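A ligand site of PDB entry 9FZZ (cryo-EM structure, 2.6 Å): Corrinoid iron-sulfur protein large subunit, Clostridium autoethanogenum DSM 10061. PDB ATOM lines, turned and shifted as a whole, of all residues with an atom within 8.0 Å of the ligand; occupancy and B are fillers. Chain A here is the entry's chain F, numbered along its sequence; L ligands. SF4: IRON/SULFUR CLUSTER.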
ATOM      1  N   PHE A   9      -2.713  10.362 -21.312  1.00  0.00           N
ATOM      2  CA  PHE A   9      -2.129   9.575 -22.399  1.00  0.00           C
ATOM      3  C   PHE A   9      -1.932  10.417 -23.645  1.00  0.00           C
ATOM      4  O   PHE A   9      -0.962  10.225 -24.379  1.00  0.00           O
ATOM      5  CB  PHE A   9      -2.971   8.351 -22.749  1.00  0.00           C
ATOM      6  CG  PHE A   9      -2.439   7.565 -23.922  1.00  0.00           C
ATOM      7  CD1 PHE A   9      -1.413   6.634 -23.756  1.00  0.00           C
ATOM      8  CD2 PHE A   9      -2.938   7.790 -25.209  1.00  0.00           C
ATOM      9  CE1 PHE A   9      -0.893   5.915 -24.851  1.00  0.00           C
ATOM     10  CE2 PHE A   9      -2.440   7.087 -26.317  1.00  0.00           C
ATOM     11  CZ  PHE A   9      -1.401   6.138 -26.134  1.00  0.00           C
ATOM     12  N   THR A  12       1.376  12.130 -23.446  1.00  0.00           N
ATOM     13  CA  THR A  12       2.557  11.275 -23.369  1.00  0.00           C
ATOM     14  C   THR A  12       3.289  11.201 -24.709  1.00  0.00           C
ATOM     15  O   THR A  12       2.683  11.387 -25.766  1.00  0.00           O
ATOM     16  CB  THR A  12       2.195   9.867 -22.923  1.00  0.00           C
ATOM     17  OG1 THR A  12       1.328   9.247 -23.890  1.00  0.00           O
ATOM     18  CG2 THR A  12       1.511   9.889 -21.580  1.00  0.00           C
ATOM     19  N   PRO A  13       4.609  10.971 -24.685  1.00  0.00           N
ATOM     20  CA  PRO A  13       5.361  10.878 -25.944  1.00  0.00           C
ATOM     21  C   PRO A  13       4.967   9.724 -26.838  1.00  0.00           C
ATOM     22  O   PRO A  13       5.233   9.782 -28.048  1.00  0.00           O
ATOM     23  CB  PRO A  13       6.810  10.653 -25.462  1.00  0.00           C
ATOM     24  CG  PRO A  13       6.830  11.068 -23.999  1.00  0.00           C
ATOM     25  CD  PRO A  13       5.454  10.680 -23.510  1.00  0.00           C
ATOM     26  N   LYS A  14       4.354   8.689 -26.292  1.00  0.00           N
ATOM     27  CA  LYS A  14       3.872   7.543 -27.057  1.00  0.00           C
ATOM     28  C   LYS A  14       5.002   6.789 -27.747  1.00  0.00           C
ATOM     29  O   LYS A  14       4.767   6.080 -28.736  1.00  0.00           O
ATOM     30  CB  LYS A  14       2.818   7.979 -28.080  1.00  0.00           C
ATOM     31  CG  LYS A  14       1.635   8.712 -27.440  1.00  0.00           C
ATOM     32  CD  LYS A  14       0.781   9.438 -28.477  1.00  0.00           C
ATOM     33  CE  LYS A  14      -0.297  10.294 -27.796  1.00  0.00           C
ATOM     34  NZ  LYS A  14      -1.101  11.100 -28.785  1.00  0.00           N
ATOM     35  N   LYS A  15       6.231   6.905 -27.232  1.00  0.00           N
ATOM     36  CA  LYS A  15       7.347   6.156 -27.828  1.00  0.00           C
ATOM     37  C   LYS A  15       7.312   4.687 -27.463  1.00  0.00           C
ATOM     38  O   LYS A  15       7.845   3.859 -28.203  1.00  0.00           O
ATOM     39  CB  LYS A  15       8.686   6.778 -27.412  1.00  0.00           C
ATOM     40  CG  LYS A  15       9.231   7.821 -28.402  1.00  0.00           C
ATOM     41  CD  LYS A  15       8.335   9.073 -28.430  1.00  0.00           C
ATOM     42  CE  LYS A  15       8.813  10.093 -29.477  1.00  0.00           C
ATOM     43  NZ  LYS A  15      10.231  10.532 -29.216  1.00  0.00           N
ATOM     44  N   ASN A  16       6.712   4.354 -26.321  1.00  0.00           N
ATOM     45  CA  ASN A  16       6.666   2.981 -25.814  1.00  0.00           C
ATOM     46  C   ASN A  16       8.079   2.410 -25.710  1.00  0.00           C
ATOM     47  O   ASN A  16       8.363   1.274 -26.103  1.00  0.00           O
ATOM     48  CB  ASN A  16       5.783   2.100 -26.700  1.00  0.00           C
ATOM     49  CG  ASN A  16       4.326   2.547 -26.719  1.00  0.00           C
ATOM     50  OD1 ASN A  16       3.826   3.058 -25.729  1.00  0.00           O
ATOM     51  ND2 ASN A  16       3.647   2.351 -27.849  1.00  0.00           N
ATOM     52  N   CYS A  17       8.985   3.222 -25.162  1.00  0.00           N
ATOM     53  CA  CYS A  17      10.396   2.856 -25.061  1.00  0.00           C
ATOM     54  C   CYS A  17      10.691   1.946 -23.884  1.00  0.00           C
ATOM     55  O   CYS A  17      11.819   1.447 -23.774  1.00  0.00           O
ATOM     56  CB  CYS A  17      11.285   4.107 -25.000  1.00  0.00           C
ATOM     57  SG  CYS A  17      10.954   5.197 -23.644  1.00  0.00           S
ATOM     58  N   LYS A  18       9.718   1.725 -22.997  1.00  0.00           N
ATOM     59  CA  LYS A  18       9.887   0.870 -21.820  1.00  0.00           C
ATOM     60  C   LYS A  18      10.970   1.383 -20.879  1.00  0.00           C
ATOM     61  O   LYS A  18      11.485   0.622 -20.047  1.00  0.00           O
ATOM     62  CB  LYS A  18      10.213  -0.573 -22.221  1.00  0.00           C
ATOM     63  CG  LYS A  18       9.253  -1.180 -23.234  1.00  0.00           C
ATOM     64  CD  LYS A  18       9.616  -2.640 -23.519  1.00  0.00           C
ATOM     65  CE  LYS A  18       8.703  -3.246 -24.598  1.00  0.00           C
ATOM     66  NZ  LYS A  18       7.260  -3.269 -24.148  1.00  0.00           N
ATOM     67  N   ASP A  19      11.337   2.661 -20.976  1.00  0.00           N
ATOM     68  CA  ASP A  19      12.374   3.206 -20.115  1.00  0.00           C
ATOM     69  C   ASP A  19      11.879   3.554 -18.718  1.00  0.00           C
ATOM     70  O   ASP A  19      12.695   3.756 -17.819  1.00  0.00           O
ATOM     71  CB  ASP A  19      12.995   4.450 -20.758  1.00  0.00           C
ATOM     72  CG  ASP A  19      13.879   4.119 -21.951  1.00  0.00           C
ATOM     73  OD1 ASP A  19      14.186   2.931 -22.129  1.00  0.00           O
ATOM     74  OD2 ASP A  19      14.248   5.036 -22.707  1.00  0.00           O
ATOM     75  N   CYS A  20      10.568   3.627 -18.513  1.00  0.00           N
ATOM     76  CA  CYS A  20       9.977   3.906 -17.209  1.00  0.00           C
ATOM     77  C   CYS A  20       9.643   2.628 -16.454  1.00  0.00           C
ATOM     78  O   CYS A  20       9.014   2.701 -15.395  1.00  0.00           O
ATOM     79  CB  CYS A  20       8.735   4.790 -17.327  1.00  0.00           C
ATOM     80  SG  CYS A  20       7.468   4.130 -18.415  1.00  0.00           S
ATOM     81  N   GLY A  21      10.027   1.466 -16.980  1.00  0.00           N
ATOM     82  CA  GLY A  21       9.640   0.201 -16.377  1.00  0.00           C
ATOM     83  C   GLY A  21       8.289  -0.301 -16.786  1.00  0.00           C
ATOM     84  O   GLY A  21       7.912  -1.414 -16.399  1.00  0.00           O
ATOM     85  N   PHE A  22       7.527   0.478 -17.560  1.00  0.00           N
ATOM     86  CA  PHE A  22       6.205   0.107 -18.036  1.00  0.00           C
ATOM     87  C   PHE A  22       6.240  -0.132 -19.538  1.00  0.00           C
ATOM     88  O   PHE A  22       6.754   0.724 -20.280  1.00  0.00           O
ATOM     89  CB  PHE A  22       5.197   1.213 -17.704  1.00  0.00           C
ATOM     90  CG  PHE A  22       5.100   1.510 -16.233  1.00  0.00           C
ATOM     91  CD1 PHE A  22       5.172   0.478 -15.297  1.00  0.00           C
ATOM     92  CD2 PHE A  22       4.961   2.819 -15.788  1.00  0.00           C
ATOM     93  CE1 PHE A  22       5.093   0.741 -13.921  1.00  0.00           C
ATOM     94  CE2 PHE A  22       4.877   3.112 -14.411  1.00  0.00           C
ATOM     95  CZ  PHE A  22       4.950   2.069 -13.476  1.00  0.00           C
ATOM     96  N   PRO A  23       5.718  -1.253 -20.021  1.00  0.00           N
ATOM     97  CA  PRO A  23       5.905  -1.595 -21.442  1.00  0.00           C
ATOM     98  C   PRO A  23       5.321  -0.578 -22.416  1.00  0.00           C
ATOM     99  O   PRO A  23       5.894  -0.386 -23.490  1.00  0.00           O
ATOM    100  CB  PRO A  23       5.236  -2.971 -21.574  1.00  0.00           C
ATOM    101  CG  PRO A  23       4.289  -3.072 -20.387  1.00  0.00           C
ATOM    102  CD  PRO A  23       4.959  -2.294 -19.285  1.00  0.00           C
ATOM    103  N   THR A  24       4.217   0.077 -22.072  1.00  0.00           N
ATOM    104  CA  THR A  24       3.559   1.005 -22.983  1.00  0.00           C
ATOM    105  C   THR A  24       3.289   2.340 -22.280  1.00  0.00           C
ATOM    106  O   THR A  24       3.205   2.412 -21.053  1.00  0.00           O
ATOM    107  CB  THR A  24       2.243   0.442 -23.536  1.00  0.00           C
ATOM    108  OG1 THR A  24       1.520  -0.220 -22.501  1.00  0.00           O
ATOM    109  CG2 THR A  24       2.530  -0.530 -24.670  1.00  0.00           C
ATOM    110  N   CYS A  25       3.170   3.390 -23.096  1.00  0.00           N
ATOM    111  CA  CYS A  25       2.832   4.694 -22.547  1.00  0.00           C
ATOM    112  C   CYS A  25       1.452   4.700 -21.930  1.00  0.00           C
ATOM    113  O   CYS A  25       1.191   5.448 -20.990  1.00  0.00           O
ATOM    114  CB  CYS A  25       2.911   5.773 -23.644  1.00  0.00           C
ATOM    115  SG  CYS A  25       4.544   6.505 -23.836  1.00  0.00           S
ATOM    116  N   LEU A  26       0.532   3.884 -22.461  1.00  0.00           N
ATOM    117  CA  LEU A  26      -0.783   3.782 -21.854  1.00  0.00           C
ATOM    118  C   LEU A  26      -0.692   3.181 -20.461  1.00  0.00           C
ATOM    119  O   LEU A  26      -1.391   3.621 -19.539  1.00  0.00           O
ATOM    120  CB  LEU A  26      -1.705   2.934 -22.735  1.00  0.00           C
ATOM    121  CG  LEU A  26      -3.192   2.975 -22.369  1.00  0.00           C
ATOM    122  CD1 LEU A  26      -3.908   4.091 -23.123  1.00  0.00           C
ATOM    123  CD2 LEU A  26      -3.836   1.628 -22.647  1.00  0.00           C
ATOM    124  N   ALA A  27       0.165   2.182 -20.278  1.00  0.00           N
ATOM    125  CA  ALA A  27       0.356   1.595 -18.955  1.00  0.00           C
ATOM    126  C   ALA A  27       0.904   2.616 -17.968  1.00  0.00           C
ATOM    127  O   ALA A  27       0.431   2.720 -16.829  1.00  0.00           O
ATOM    128  CB  ALA A  27       1.279   0.382 -19.041  1.00  0.00           C
ATOM    129  N   PHE A  28       1.892   3.400 -18.394  1.00  0.00           N
ATOM    130  CA  PHE A  28       2.437   4.455 -17.541  1.00  0.00           C
ATOM    131  C   PHE A  28       1.363   5.486 -17.217  1.00  0.00           C
ATOM    132  O   PHE A  28       1.245   5.941 -16.069  1.00  0.00           O
ATOM    133  CB  PHE A  28       3.644   5.099 -18.214  1.00  0.00           C
ATOM    134  CG  PHE A  28       4.122   6.359 -17.543  1.00  0.00           C
ATOM    135  CD1 PHE A  28       4.960   6.283 -16.424  1.00  0.00           C
ATOM    136  CD2 PHE A  28       3.745   7.611 -18.022  1.00  0.00           C
ATOM    137  CE1 PHE A  28       5.405   7.444 -15.775  1.00  0.00           C
ATOM    138  CE2 PHE A  28       4.177   8.791 -17.391  1.00  0.00           C
ATOM    139  CZ  PHE A  28       5.015   8.715 -16.271  1.00  0.00           C
ATOM    140  N   SER A  29       0.570   5.875 -18.214  1.00  0.00           N
ATOM    141  CA  SER A  29      -0.482   6.863 -18.007  1.00  0.00           C
ATOM    142  C   SER A  29      -1.515   6.350 -17.005  1.00  0.00           C
ATOM    143  O   SER A  29      -1.935   7.095 -16.113  1.00  0.00           O
ATOM    144  CB  SER A  29      -1.125   7.191 -19.356  1.00  0.00           C
ATOM    145  OG  SER A  29      -2.421   7.760 -19.216  1.00  0.00           O
ATOM    146  N   VAL A  32       0.123   6.398 -13.405  1.00  0.00           N
ATOM    147  CA  VAL A  32       0.136   7.724 -12.799  1.00  0.00           C
ATOM    148  C   VAL A  32      -1.274   8.267 -12.604  1.00  0.00           C
ATOM    149  O   VAL A  32      -1.470   9.175 -11.784  1.00  0.00           O
ATOM    150  CB  VAL A  32       0.989   8.715 -13.598  1.00  0.00           C
ATOM    151  CG1 VAL A  32       2.370   8.128 -13.898  1.00  0.00           C
ATOM    152  CG2 VAL A  32       0.284   9.111 -14.879  1.00  0.00           C
ATOM    153  N   ILE A  39       4.458  11.705 -12.086  1.00  0.00           N
ATOM    154  CA  ILE A  39       4.682  11.771 -13.521  1.00  0.00           C
ATOM    155  C   ILE A  39       6.143  11.980 -13.893  1.00  0.00           C
ATOM    156  O   ILE A  39       6.509  11.824 -15.067  1.00  0.00           O
ATOM    157  CB  ILE A  39       3.798  12.868 -14.139  1.00  0.00           C
ATOM    158  CG1 ILE A  39       3.963  12.903 -15.666  1.00  0.00           C
ATOM    159  CG2 ILE A  39       4.119  14.229 -13.514  1.00  0.00           C
ATOM    160  CD1 ILE A  39       3.122  13.948 -16.334  1.00  0.00           C
ATOM    161  N   LYS A  41       8.556  10.170 -13.799  1.00  0.00           N
ATOM    162  CA  LYS A  41       9.249   8.958 -14.199  1.00  0.00           C
ATOM    163  C   LYS A  41       9.548   8.878 -15.690  1.00  0.00           C
ATOM    164  O   LYS A  41      10.385   8.065 -16.097  1.00  0.00           O
ATOM    165  CB  LYS A  41       8.421   7.727 -13.770  1.00  0.00           C
ATOM    166  CG  LYS A  41       8.884   7.085 -12.447  1.00  0.00           C
ATOM    167  CD  LYS A  41      10.356   6.603 -12.531  1.00  0.00           C
ATOM    168  CE  LYS A  41      10.559   5.572 -13.656  1.00  0.00           C
ATOM    169  NZ  LYS A  41      11.962   5.599 -14.187  1.00  0.00           N
ATOM    170  N   CYS A  42       8.891   9.681 -16.515  1.00  0.00           N
ATOM    171  CA  CYS A  42       9.069   9.583 -17.960  1.00  0.00           C
ATOM    172  C   CYS A  42      10.207  10.503 -18.410  1.00  0.00           C
ATOM    173  O   CYS A  42      10.077  11.719 -18.272  1.00  0.00           O
ATOM    174  CB  CYS A  42       7.776   9.940 -18.668  1.00  0.00           C
ATOM    175  SG  CYS A  42       7.863   9.730 -20.427  1.00  0.00           S
ATOM    176  N   PRO A  43      11.309   9.965 -18.960  1.00  0.00           N
ATOM    177  CA  PRO A  43      12.424  10.858 -19.354  1.00  0.00           C
ATOM    178  C   PRO A  43      12.147  11.671 -20.610  1.00  0.00           C
ATOM    179  O   PRO A  43      12.757  12.736 -20.770  1.00  0.00           O
ATOM    180  CB  PRO A  43      13.610   9.889 -19.558  1.00  0.00           C
ATOM    181  CG  PRO A  43      13.165   8.550 -18.945  1.00  0.00           C
ATOM    182  CD  PRO A  43      11.675   8.543 -19.105  1.00  0.00           C
ATOM    183  N   HIS A  44      11.251  11.217 -21.487  1.00  0.00           N
ATOM    184  CA  HIS A  44      11.054  11.834 -22.787  1.00  0.00           C
ATOM    185  C   HIS A  44       9.866  12.799 -22.825  1.00  0.00           C
ATOM    186  O   HIS A  44       9.516  13.285 -23.891  1.00  0.00           O
ATOM    187  CB  HIS A  44      10.864  10.748 -23.858  1.00  0.00           C
ATOM    188  CG  HIS A  44      11.904   9.659 -23.809  1.00  0.00           C
ATOM    189  ND1 HIS A  44      11.940   8.700 -22.840  1.00  0.00           N
ATOM    190  CD2 HIS A  44      12.958   9.405 -24.633  1.00  0.00           C
ATOM    191  CE1 HIS A  44      12.955   7.889 -23.042  1.00  0.00           C
ATOM    192  NE2 HIS A  44      13.587   8.298 -24.127  1.00  0.00           N
ATOM    193  N   MET A  45       9.253  13.087 -21.678  1.00  0.00           N
ATOM    194  CA  MET A  45       8.088  13.964 -21.665  1.00  0.00           C
ATOM    195  C   MET A  45       8.474  15.368 -22.133  1.00  0.00           C
ATOM    196  O   MET A  45       9.518  15.897 -21.761  1.00  0.00           O
ATOM    197  CB  MET A  45       7.490  14.044 -20.256  1.00  0.00           C
ATOM    198  CG  MET A  45       6.511  12.925 -19.898  1.00  0.00           C
ATOM    199  SD  MET A  45       4.938  13.053 -20.757  1.00  0.00           S
ATOM    200  CE  MET A  45       4.320  14.646 -20.232  1.00  0.00           C
HETATM  201 FE1  SF4 L   1       7.797   7.774 -21.249  1.00  0.00          FE
HETATM  202 FE2  SF4 L   1       6.422   5.892 -22.641  1.00  0.00          FE
HETATM  203 FE3  SF4 L   1       7.776   5.199 -20.358  1.00  0.00          FE
HETATM  204 FE4  SF4 L   1       9.152   5.870 -22.624  1.00  0.00          FE
HETATM  205  S1  SF4 L   1       7.779   4.076 -22.344  1.00  0.00           S
HETATM  206  S2  SF4 L   1       9.583   6.570 -20.500  1.00  0.00           S
HETATM  207  S3  SF4 L   1       7.802   7.487 -23.496  1.00  0.00           S
HETATM  208  S4  SF4 L   1       5.987   6.601 -20.524  1.00  0.00           S
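A ring nitrogen (ND1) of His 44 sits close to the side-chain sulfur of Cys 17. OD2 of Asp 19 lies close to SG of Cys 17, at 3.4 Å. The side-chain sulfur (SG) of Cys 20 lies close to the backbone NH (N) of Phe 22. The backbone NH (N) of Cys 25 sits at hydrogen-bond distance from the side-chain amide oxygen (OD1) of Asn 16 (2.7 Å). SG of Cys 25 sits close to N of Lys 14 (3.3 Å). NZ of Lys 18 is in hydrogen-bond range of O of Pro 23 (3.3 Å).
The side-chain sulfur of Cys 42 is bound to an iron atom (FE1) of the ligand (2.1 Å). N of Cys 17 sits close to S1 of the ligand, 3.2 Å away. The side-chain sulfur (SG) of Cys 17 binds an iron atom (FE4) of the ligand (2.2 Å). The backbone NH of Cys 20 lies close to a sulfur (S2) of the ligand, 3.7 Å away. The side-chain sulfur (SG) of Cys 20 binds an iron atom (FE3) of the ligand (2.2 Å). The side-chain sulfur of Cys 25 binds an iron atom (FE2) of the ligand (2.3 Å). S1 of the ligand sits close to N of Lys 18, at 3.1 Å.
Residues that only touch the ligand: Pro 13, Asn 16, Phe 28, Pro 43 and His 44. Within 4 Å of the ligand: Pro 13, Asn 16, Cys 17, Lys 18, Cys 20, Cys 25, Phe 28, Cys 42, Pro 43 and His 44. The nearest printed residue that does not touch the ligand is Asp 19 (4.03 Å).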
